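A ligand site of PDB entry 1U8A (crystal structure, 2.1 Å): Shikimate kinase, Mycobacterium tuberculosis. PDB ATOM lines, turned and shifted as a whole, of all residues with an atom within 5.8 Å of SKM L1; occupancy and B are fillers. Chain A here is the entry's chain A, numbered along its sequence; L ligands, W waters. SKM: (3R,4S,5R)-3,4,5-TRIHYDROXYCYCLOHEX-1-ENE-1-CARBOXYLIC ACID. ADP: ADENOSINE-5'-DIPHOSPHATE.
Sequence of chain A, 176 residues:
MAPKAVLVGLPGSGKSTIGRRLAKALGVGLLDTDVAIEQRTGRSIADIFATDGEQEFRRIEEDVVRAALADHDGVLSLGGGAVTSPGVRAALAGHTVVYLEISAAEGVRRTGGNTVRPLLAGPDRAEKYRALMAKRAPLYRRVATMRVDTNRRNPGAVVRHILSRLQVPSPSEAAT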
ATOM      1  N   PRO A  11      22.596 -21.202  18.170  1.00  0.00           N
ATOM      2  CA  PRO A  11      22.956 -19.814  17.875  1.00  0.00           C
ATOM      3  C   PRO A  11      23.150 -19.148  19.226  1.00  0.00           C
ATOM      4  O   PRO A  11      22.339 -19.346  20.127  1.00  0.00           O
ATOM      5  CB  PRO A  11      21.712 -19.288  17.183  1.00  0.00           C
ATOM      6  CG  PRO A  11      21.120 -20.496  16.545  1.00  0.00           C
ATOM      7  CD  PRO A  11      21.280 -21.538  17.608  1.00  0.00           C
ATOM      8  N   LYS A  15      30.040 -20.038  19.170  1.00  0.00           N
ATOM      9  CA  LYS A  15      30.891 -20.561  18.097  1.00  0.00           C
ATOM     10  C   LYS A  15      31.841 -19.523  17.496  1.00  0.00           C
ATOM     11  O   LYS A  15      33.043 -19.719  17.423  1.00  0.00           O
ATOM     12  CB  LYS A  15      30.040 -21.169  16.979  1.00  0.00           C
ATOM     13  CG  LYS A  15      29.116 -22.301  17.433  1.00  0.00           C
ATOM     14  CD  LYS A  15      28.254 -22.815  16.272  1.00  0.00           C
ATOM     15  CE  LYS A  15      27.191 -21.789  15.843  1.00  0.00           C
ATOM     16  NZ  LYS A  15      26.104 -21.673  16.844  1.00  0.00           N
ATOM     17  N   ASP A  34      29.876 -19.894   8.205  1.00  0.00           N
ATOM     18  CA  ASP A  34      28.890 -18.905   7.778  1.00  0.00           C
ATOM     19  C   ASP A  34      29.589 -17.822   6.965  1.00  0.00           C
ATOM     20  O   ASP A  34      29.156 -17.466   5.870  1.00  0.00           O
ATOM     21  CB  ASP A  34      28.184 -18.275   8.980  1.00  0.00           C
ATOM     22  CG  ASP A  34      27.129 -19.180   9.585  1.00  0.00           C
ATOM     23  OD1 ASP A  34      26.518 -19.965   8.818  1.00  0.00           O
ATOM     24  OD2 ASP A  34      26.896 -19.087  10.806  1.00  0.00           O
ATOM     25  N   ILE A  45      23.746 -14.633   4.329  1.00  0.00           N
ATOM     26  CA  ILE A  45      23.029 -15.845   4.683  1.00  0.00           C
ATOM     27  C   ILE A  45      21.532 -15.575   4.755  1.00  0.00           C
ATOM     28  O   ILE A  45      20.731 -16.368   4.279  1.00  0.00           O
ATOM     29  CB  ILE A  45      23.516 -16.408   6.046  1.00  0.00           C
ATOM     30  CG1 ILE A  45      25.011 -16.729   5.975  1.00  0.00           C
ATOM     31  CG2 ILE A  45      22.717 -17.636   6.429  1.00  0.00           C
ATOM     32  CD1 ILE A  45      25.421 -17.472   4.716  1.00  0.00           C
ATOM     33  N   PHE A  49      18.673 -17.524   2.434  1.00  0.00           N
ATOM     34  CA  PHE A  49      17.526 -18.156   3.073  1.00  0.00           C
ATOM     35  C   PHE A  49      16.230 -17.748   2.380  1.00  0.00           C
ATOM     36  O   PHE A  49      15.438 -18.584   1.963  1.00  0.00           O
ATOM     37  CB  PHE A  49      17.463 -17.757   4.542  1.00  0.00           C
ATOM     38  CG  PHE A  49      18.032 -18.788   5.490  1.00  0.00           C
ATOM     39  CD1 PHE A  49      17.303 -19.922   5.814  1.00  0.00           C
ATOM     40  CD2 PHE A  49      19.279 -18.609   6.064  1.00  0.00           C
ATOM     41  CE1 PHE A  49      17.809 -20.872   6.702  1.00  0.00           C
ATOM     42  CE2 PHE A  49      19.806 -19.551   6.947  1.00  0.00           C
ATOM     43  CZ  PHE A  49      19.065 -20.688   7.267  1.00  0.00           C
ATOM     44  N   GLU A  54      16.272 -23.191   3.100  1.00  0.00           N
ATOM     45  CA  GLU A  54      17.233 -24.015   3.824  1.00  0.00           C
ATOM     46  C   GLU A  54      17.888 -25.125   3.015  1.00  0.00           C
ATOM     47  O   GLU A  54      19.120 -25.181   2.923  1.00  0.00           O
ATOM     48  CB  GLU A  54      16.586 -24.631   5.065  1.00  0.00           C
ATOM     49  CG  GLU A  54      16.759 -23.800   6.318  1.00  0.00           C
ATOM     50  CD  GLU A  54      16.626 -24.604   7.594  1.00  0.00           C
ATOM     51  OE1 GLU A  54      17.311 -25.632   7.723  1.00  0.00           O
ATOM     52  OE2 GLU A  54      15.819 -24.206   8.466  1.00  0.00           O
ATOM     53  N   PHE A  57      20.639 -23.698   1.346  1.00  0.00           N
ATOM     54  CA  PHE A  57      21.700 -23.169   2.208  1.00  0.00           C
ATOM     55  C   PHE A  57      22.462 -24.349   2.798  1.00  0.00           C
ATOM     56  O   PHE A  57      23.685 -24.299   2.931  1.00  0.00           O
ATOM     57  CB  PHE A  57      21.122 -22.336   3.342  1.00  0.00           C
ATOM     58  CG  PHE A  57      22.153 -21.880   4.336  1.00  0.00           C
ATOM     59  CD1 PHE A  57      23.048 -20.867   4.021  1.00  0.00           C
ATOM     60  CD2 PHE A  57      22.255 -22.498   5.585  1.00  0.00           C
ATOM     61  CE1 PHE A  57      24.028 -20.466   4.933  1.00  0.00           C
ATOM     62  CE2 PHE A  57      23.235 -22.105   6.503  1.00  0.00           C
ATOM     63  CZ  PHE A  57      24.126 -21.082   6.169  1.00  0.00           C
ATOM     64  N   ARG A  58      21.734 -25.410   3.132  1.00  0.00           N
ATOM     65  CA  ARG A  58      22.326 -26.601   3.709  1.00  0.00           C
ATOM     66  C   ARG A  58      23.258 -27.338   2.755  1.00  0.00           C
ATOM     67  O   ARG A  58      24.300 -27.843   3.173  1.00  0.00           O
ATOM     68  CB  ARG A  58      21.242 -27.552   4.227  1.00  0.00           C
ATOM     69  CG  ARG A  58      20.368 -26.959   5.338  1.00  0.00           C
ATOM     70  CD  ARG A  58      21.202 -26.422   6.496  1.00  0.00           C
ATOM     71  NE  ARG A  58      20.392 -25.791   7.542  1.00  0.00           N
ATOM     72  CZ  ARG A  58      20.889 -25.055   8.534  1.00  0.00           C
ATOM     73  NH1 ARG A  58      22.187 -24.847   8.638  1.00  0.00           N
ATOM     74  NH2 ARG A  58      20.070 -24.530   9.434  1.00  0.00           N
ATOM     75  N   GLU A  61      26.340 -25.047   2.537  1.00  0.00           N
ATOM     76  CA  GLU A  61      27.008 -25.185   3.818  1.00  0.00           C
ATOM     77  C   GLU A  61      27.762 -26.513   3.863  1.00  0.00           C
ATOM     78  O   GLU A  61      28.973 -26.533   4.116  1.00  0.00           O
ATOM     79  CB  GLU A  61      25.957 -25.116   4.936  1.00  0.00           C
ATOM     80  CG  GLU A  61      26.489 -25.291   6.362  1.00  0.00           C
ATOM     81  CD  GLU A  61      25.410 -25.122   7.413  1.00  0.00           C
ATOM     82  OE1 GLU A  61      24.459 -25.940   7.429  1.00  0.00           O
ATOM     83  OE2 GLU A  61      25.507 -24.169   8.231  1.00  0.00           O
ATOM     84  N   LEU A  78      31.296 -24.004  12.790  1.00  0.00           N
ATOM     85  CA  LEU A  78      30.184 -24.296  11.887  1.00  0.00           C
ATOM     86  C   LEU A  78      28.978 -23.413  12.169  1.00  0.00           C
ATOM     87  O   LEU A  78      28.845 -22.840  13.251  1.00  0.00           O
ATOM     88  CB  LEU A  78      29.734 -25.752  12.020  1.00  0.00           C
ATOM     89  CG  LEU A  78      30.761 -26.876  12.045  1.00  0.00           C
ATOM     90  CD1 LEU A  78      30.027 -28.208  11.905  1.00  0.00           C
ATOM     91  CD2 LEU A  78      31.756 -26.700  10.896  1.00  0.00           C
ATOM     92  N   GLY A  79      28.090 -23.328  11.187  1.00  0.00           N
ATOM     93  CA  GLY A  79      26.876 -22.555  11.367  1.00  0.00           C
ATOM     94  C   GLY A  79      26.035 -23.331  12.367  1.00  0.00           C
ATOM     95  O   GLY A  79      26.092 -24.555  12.417  1.00  0.00           O
ATOM     96  N   GLY A  80      25.226 -22.610  13.143  1.00  0.00           N
ATOM     97  CA  GLY A  80      24.395 -23.243  14.160  1.00  0.00           C
ATOM     98  C   GLY A  80      23.634 -24.501  13.778  1.00  0.00           C
ATOM     99  O   GLY A  80      23.486 -25.399  14.608  1.00  0.00           O
ATOM    100  N   GLY A  81      23.145 -24.578  12.550  1.00  0.00           N
ATOM    101  CA  GLY A  81      22.381 -25.738  12.145  1.00  0.00           C
ATOM    102  C   GLY A  81      23.042 -26.684  11.157  1.00  0.00           C
ATOM    103  O   GLY A  81      22.350 -27.483  10.516  1.00  0.00           O
ATOM    104  N   ALA A  82      24.359 -26.615  11.029  1.00  0.00           N
ATOM    105  CA  ALA A  82      25.055 -27.493  10.092  1.00  0.00           C
ATOM    106  C   ALA A  82      24.842 -28.964  10.474  1.00  0.00           C
ATOM    107  O   ALA A  82      24.686 -29.823   9.598  1.00  0.00           O
ATOM    108  CB  ALA A  82      26.560 -27.166  10.072  1.00  0.00           C
ATOM    109  N   VAL A 116      22.502 -11.436  11.836  1.00  0.00           N
ATOM    110  CA  VAL A 116      21.123 -11.766  12.183  1.00  0.00           C
ATOM    111  C   VAL A 116      20.819 -13.219  11.830  1.00  0.00           C
ATOM    112  O   VAL A 116      21.391 -13.784  10.898  1.00  0.00           O
ATOM    113  CB  VAL A 116      20.129 -10.838  11.476  1.00  0.00           C
ATOM    114  CG1 VAL A 116      18.913 -11.576  11.008  1.00  0.00           C
ATOM    115  CG2 VAL A 116      19.739  -9.707  12.420  1.00  0.00           C
ATOM    116  N   ARG A 117      19.900 -13.797  12.597  1.00  0.00           N
ATOM    117  CA  ARG A 117      19.418 -15.180  12.505  1.00  0.00           C
ATOM    118  C   ARG A 117      18.044 -15.356  11.870  1.00  0.00           C
ATOM    119  O   ARG A 117      17.033 -14.949  12.438  1.00  0.00           O
ATOM    120  CB  ARG A 117      19.339 -15.780  13.920  1.00  0.00           C
ATOM    121  CG  ARG A 117      20.548 -16.540  14.389  1.00  0.00           C
ATOM    122  CD  ARG A 117      21.853 -15.831  14.079  1.00  0.00           C
ATOM    123  NE  ARG A 117      22.884 -16.096  15.076  1.00  0.00           N
ATOM    124  CZ  ARG A 117      22.920 -15.533  16.287  1.00  0.00           C
ATOM    125  NH1 ARG A 117      21.970 -14.682  16.654  1.00  0.00           N
ATOM    126  NH2 ARG A 117      23.915 -15.807  17.114  1.00  0.00           N
ATOM    127  N   PRO A 118      17.991 -15.975  10.686  1.00  0.00           N
ATOM    128  CA  PRO A 118      16.695 -16.173  10.042  1.00  0.00           C
ATOM    129  C   PRO A 118      15.744 -17.095  10.815  1.00  0.00           C
ATOM    130  O   PRO A 118      14.526 -16.884  10.828  1.00  0.00           O
ATOM    131  CB  PRO A 118      17.071 -16.753   8.681  1.00  0.00           C
ATOM    132  CG  PRO A 118      18.393 -16.131   8.391  1.00  0.00           C
ATOM    133  CD  PRO A 118      19.095 -16.016   9.713  1.00  0.00           C
ATOM    134  N   LEU A 119      16.293 -18.117  11.458  1.00  0.00           N
ATOM    135  CA  LEU A 119      15.465 -19.065  12.200  1.00  0.00           C
ATOM    136  C   LEU A 119      15.035 -18.619  13.601  1.00  0.00           C
ATOM    137  O   LEU A 119      14.036 -19.108  14.115  1.00  0.00           O
ATOM    138  CB  LEU A 119      16.171 -20.406  12.308  1.00  0.00           C
ATOM    139  CG  LEU A 119      16.592 -21.007  10.969  1.00  0.00           C
ATOM    140  CD1 LEU A 119      17.171 -22.407  11.166  1.00  0.00           C
ATOM    141  CD2 LEU A 119      15.427 -21.045   9.998  1.00  0.00           C
ATOM    142  N   LEU A 132      14.279 -25.022  18.903  1.00  0.00           N
ATOM    143  CA  LEU A 132      15.530 -25.268  18.216  1.00  0.00           C
ATOM    144  C   LEU A 132      16.388 -26.176  19.091  1.00  0.00           C
ATOM    145  O   LEU A 132      16.991 -27.136  18.606  1.00  0.00           O
ATOM    146  CB  LEU A 132      16.225 -23.917  17.983  1.00  0.00           C
ATOM    147  CG  LEU A 132      17.015 -23.690  16.692  1.00  0.00           C
ATOM    148  CD1 LEU A 132      16.092 -23.847  15.494  1.00  0.00           C
ATOM    149  CD2 LEU A 132      17.617 -22.300  16.714  1.00  0.00           C
ATOM    150  N   ARG A 136      17.748 -29.894  18.088  1.00  0.00           N
ATOM    151  CA  ARG A 136      19.161 -30.094  17.835  1.00  0.00           C
ATOM    152  C   ARG A 136      20.012 -30.669  18.958  1.00  0.00           C
ATOM    153  O   ARG A 136      21.068 -31.240  18.696  1.00  0.00           O
ATOM    154  CB  ARG A 136      19.772 -28.779  17.369  1.00  0.00           C
ATOM    155  CG  ARG A 136      19.159 -28.296  16.083  1.00  0.00           C
ATOM    156  CD  ARG A 136      19.624 -26.905  15.744  1.00  0.00           C
ATOM    157  NE  ARG A 136      19.004 -26.439  14.517  1.00  0.00           N
ATOM    158  CZ  ARG A 136      19.102 -25.196  14.061  1.00  0.00           C
ATOM    159  NH1 ARG A 136      19.786 -24.296  14.763  1.00  0.00           N
ATOM    160  NH2 ARG A 136      18.523 -24.850  12.924  1.00  0.00           N
ATOM    161  N   TYR A 140      23.885 -32.344  18.355  1.00  0.00           N
ATOM    162  CA  TYR A 140      25.164 -31.825  18.856  1.00  0.00           C
ATOM    163  C   TYR A 140      25.857 -32.883  19.705  1.00  0.00           C
ATOM    164  O   TYR A 140      27.062 -33.100  19.591  1.00  0.00           O
ATOM    165  CB  TYR A 140      24.939 -30.564  19.705  1.00  0.00           C
ATOM    166  CG  TYR A 140      24.375 -29.385  18.954  1.00  0.00           C
ATOM    167  CD1 TYR A 140      25.024 -28.873  17.839  1.00  0.00           C
ATOM    168  CD2 TYR A 140      23.188 -28.780  19.355  1.00  0.00           C
ATOM    169  CE1 TYR A 140      24.523 -27.773  17.149  1.00  0.00           C
ATOM    170  CE2 TYR A 140      22.678 -27.678  18.667  1.00  0.00           C
ATOM    171  CZ  TYR A 140      23.346 -27.186  17.559  1.00  0.00           C
ATOM    172  OH  TYR A 140      22.838 -26.106  16.860  1.00  0.00           O
HETATM  173  O12 SKM L   1      24.351 -20.646   9.957  1.00  0.00           O
HETATM  174  C8  SKM L   1      23.661 -19.458  10.357  1.00  0.00           C
HETATM  175  C6  SKM L   1      22.251 -19.472   9.748  1.00  0.00           C
HETATM  176  O7  SKM L   1      21.516 -18.332  10.183  1.00  0.00           O
HETATM  177  C5  SKM L   1      21.530 -20.767  10.159  1.00  0.00           C
HETATM  178  C4  SKM L   1      21.674 -21.074  11.662  1.00  0.00           C
HETATM  179  C1  SKM L   1      20.802 -22.179  12.291  1.00  0.00           C
HETATM  180  O2  SKM L   1      20.153 -22.997  11.531  1.00  0.00           O
HETATM  181  O3  SKM L   1      20.744 -22.321  13.571  1.00  0.00           O
HETATM  182  C10 SKM L   1      22.589 -20.463  12.436  1.00  0.00           C
HETATM  183  C9  SKM L   1      23.574 -19.402  11.895  1.00  0.00           C
HETATM  184  O11 SKM L   1      24.863 -19.610  12.471  1.00  0.00           O
HETATM  185  PB  ADP L   2      27.325 -18.155  17.728  1.00  0.00           P
HETATM  186  O1B ADP L   2      27.347 -19.512  18.312  1.00  0.00           O
HETATM  187  O2B ADP L   2      26.069 -17.591  17.067  1.00  0.00           O
HETATM  188  O3B ADP L   2      28.641 -17.882  16.790  1.00  0.00           O
HETATM  189  PA  ADP L   2      28.480 -15.838  18.961  1.00  0.00           P
HETATM  190  O1A ADP L   2      29.919 -16.262  19.033  1.00  0.00           O
HETATM  191  O2A ADP L   2      28.064 -14.856  17.889  1.00  0.00           O
HETATM  192  O3A ADP L   2      27.552 -17.096  18.865  1.00  0.00           O
HETATM  193  O5' ADP L   2      28.064 -15.297  20.431  1.00  0.00           O
HETATM  194  C5' ADP L   2      26.786 -14.540  20.560  1.00  0.00           C
HETATM  195  C4' ADP L   2      26.964 -13.450  21.656  1.00  0.00           C
HETATM  196  O4' ADP L   2      27.223 -14.034  22.962  1.00  0.00           O
HETATM  197  C3' ADP L   2      28.165 -12.500  21.468  1.00  0.00           C
HETATM  198  O3' ADP L   2      27.800 -11.093  21.627  1.00  0.00           O
HETATM  199  C2' ADP L   2      29.218 -12.890  22.501  1.00  0.00           C
HETATM  200  O2' ADP L   2      30.017 -11.787  22.961  1.00  0.00           O
HETATM  201  C1' ADP L   2      28.430 -13.496  23.598  1.00  0.00           C
HETATM  202  N9  ADP L   2      29.000 -14.683  24.338  1.00  0.00           N
HETATM  203  C8  ADP L   2      29.473 -15.865  23.727  1.00  0.00           C
HETATM  204  N7  ADP L   2      30.122 -16.619  24.601  1.00  0.00           N
HETATM  205  C5  ADP L   2      29.901 -16.037  25.836  1.00  0.00           C
HETATM  206  C6  ADP L   2      30.255 -16.422  27.180  1.00  0.00           C
HETATM  207  N6  ADP L   2      31.012 -17.482  27.491  1.00  0.00           N
HETATM  208  N1  ADP L   2      29.785 -15.606  28.229  1.00  0.00           N
HETATM  209  C2  ADP L   2      29.238 -14.363  27.920  1.00  0.00           C
HETATM  210  N3  ADP L   2      28.795 -13.923  26.691  1.00  0.00           N
HETATM  211  C4  ADP L   2      29.199 -14.834  25.684  1.00  0.00           C
HETATM  212  O   HOH W   1      19.257 -19.723  14.232  1.00  0.00           O
HETATM  213  O   HOH W   2      25.153 -17.052  14.288  1.00  0.00           O
HETATM  214  O   HOH W   3      23.804 -23.118  10.065  1.00  0.00           O
HETATM  215  O   HOH W   4      19.044 -18.676  11.753  1.00  0.00           O
HETATM  216  O   HOH W   5      24.987 -19.817  15.314  1.00  0.00           O
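The guanidinium group (NH1) of Arg 136 lies within salt-bridge range of an oxygen (O3) of SKM L1 (2.5 Å).
The side-chain carboxylate (OD1) of Asp 34 is in hydrogen-bond range of an oxygen (O12) of SKM L1 (2.5 Å).
NH2 of Arg 58 is in salt-bridge range of O2 of SKM L1 (2.6 Å).
The backbone NH (N) of Gly 80 sits at hydrogen-bond distance from an oxygen (O11) of SKM L1 (3.1 Å).
The backbone NH (N) of Gly 81 sits close to an oxygen (O3) of SKM L1.
The guanidinium group (NH2) of Arg 117 is in salt-bridge range of an oxygen (O2B) of ADP L2 (2.8 Å).
N of Lys 15 lies within hydrogen-bond range of O1B of ADP L2, 2.9 Å away.
The side-chain amino group (NZ) of Lys 15 is in salt-bridge range of an oxygen (O1B) of ADP L2, at 2.9 Å.
NH1 of Arg 58 lies close to O of Gly 81, 3.2 Å away.
OE1 of Glu 61 is in salt-bridge range of NH1 of Arg 58.
NE of Arg 58 is in salt-bridge range of OE1 of Glu 54 (3.1 Å).
The backbone carbonyl oxygen (O) of Gly 80 sits at hydrogen-bond distance from the side-chain hydroxyl (OH) of Tyr 140.
Merely in contact with SKM L1: Leu 119, Pro 118, Gly 79, Pro 11, Phe 49, Phe 57 and Ile 45.
Hydrophobic or aromatic side chains within 4 Å of SKM L1: Pro 11, Ile 45, Phe 49, Phe 57, Pro 118 and Leu 119.
Water W5 lies within hydrogen-bond range of the side-chain amino group of Lys 15, an oxygen (O11) of SKM L1 and an oxygen (O2B) of ADP L2.
Water W4 bridges N of Leu 119 and O7 of SKM L1.
Water W2 lies within hydrogen-bond range of NE of Arg 117 (2.6 Å), O2B of ADP L2 (3.0 Å) and O11 of SKM L1 (3.2 Å).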
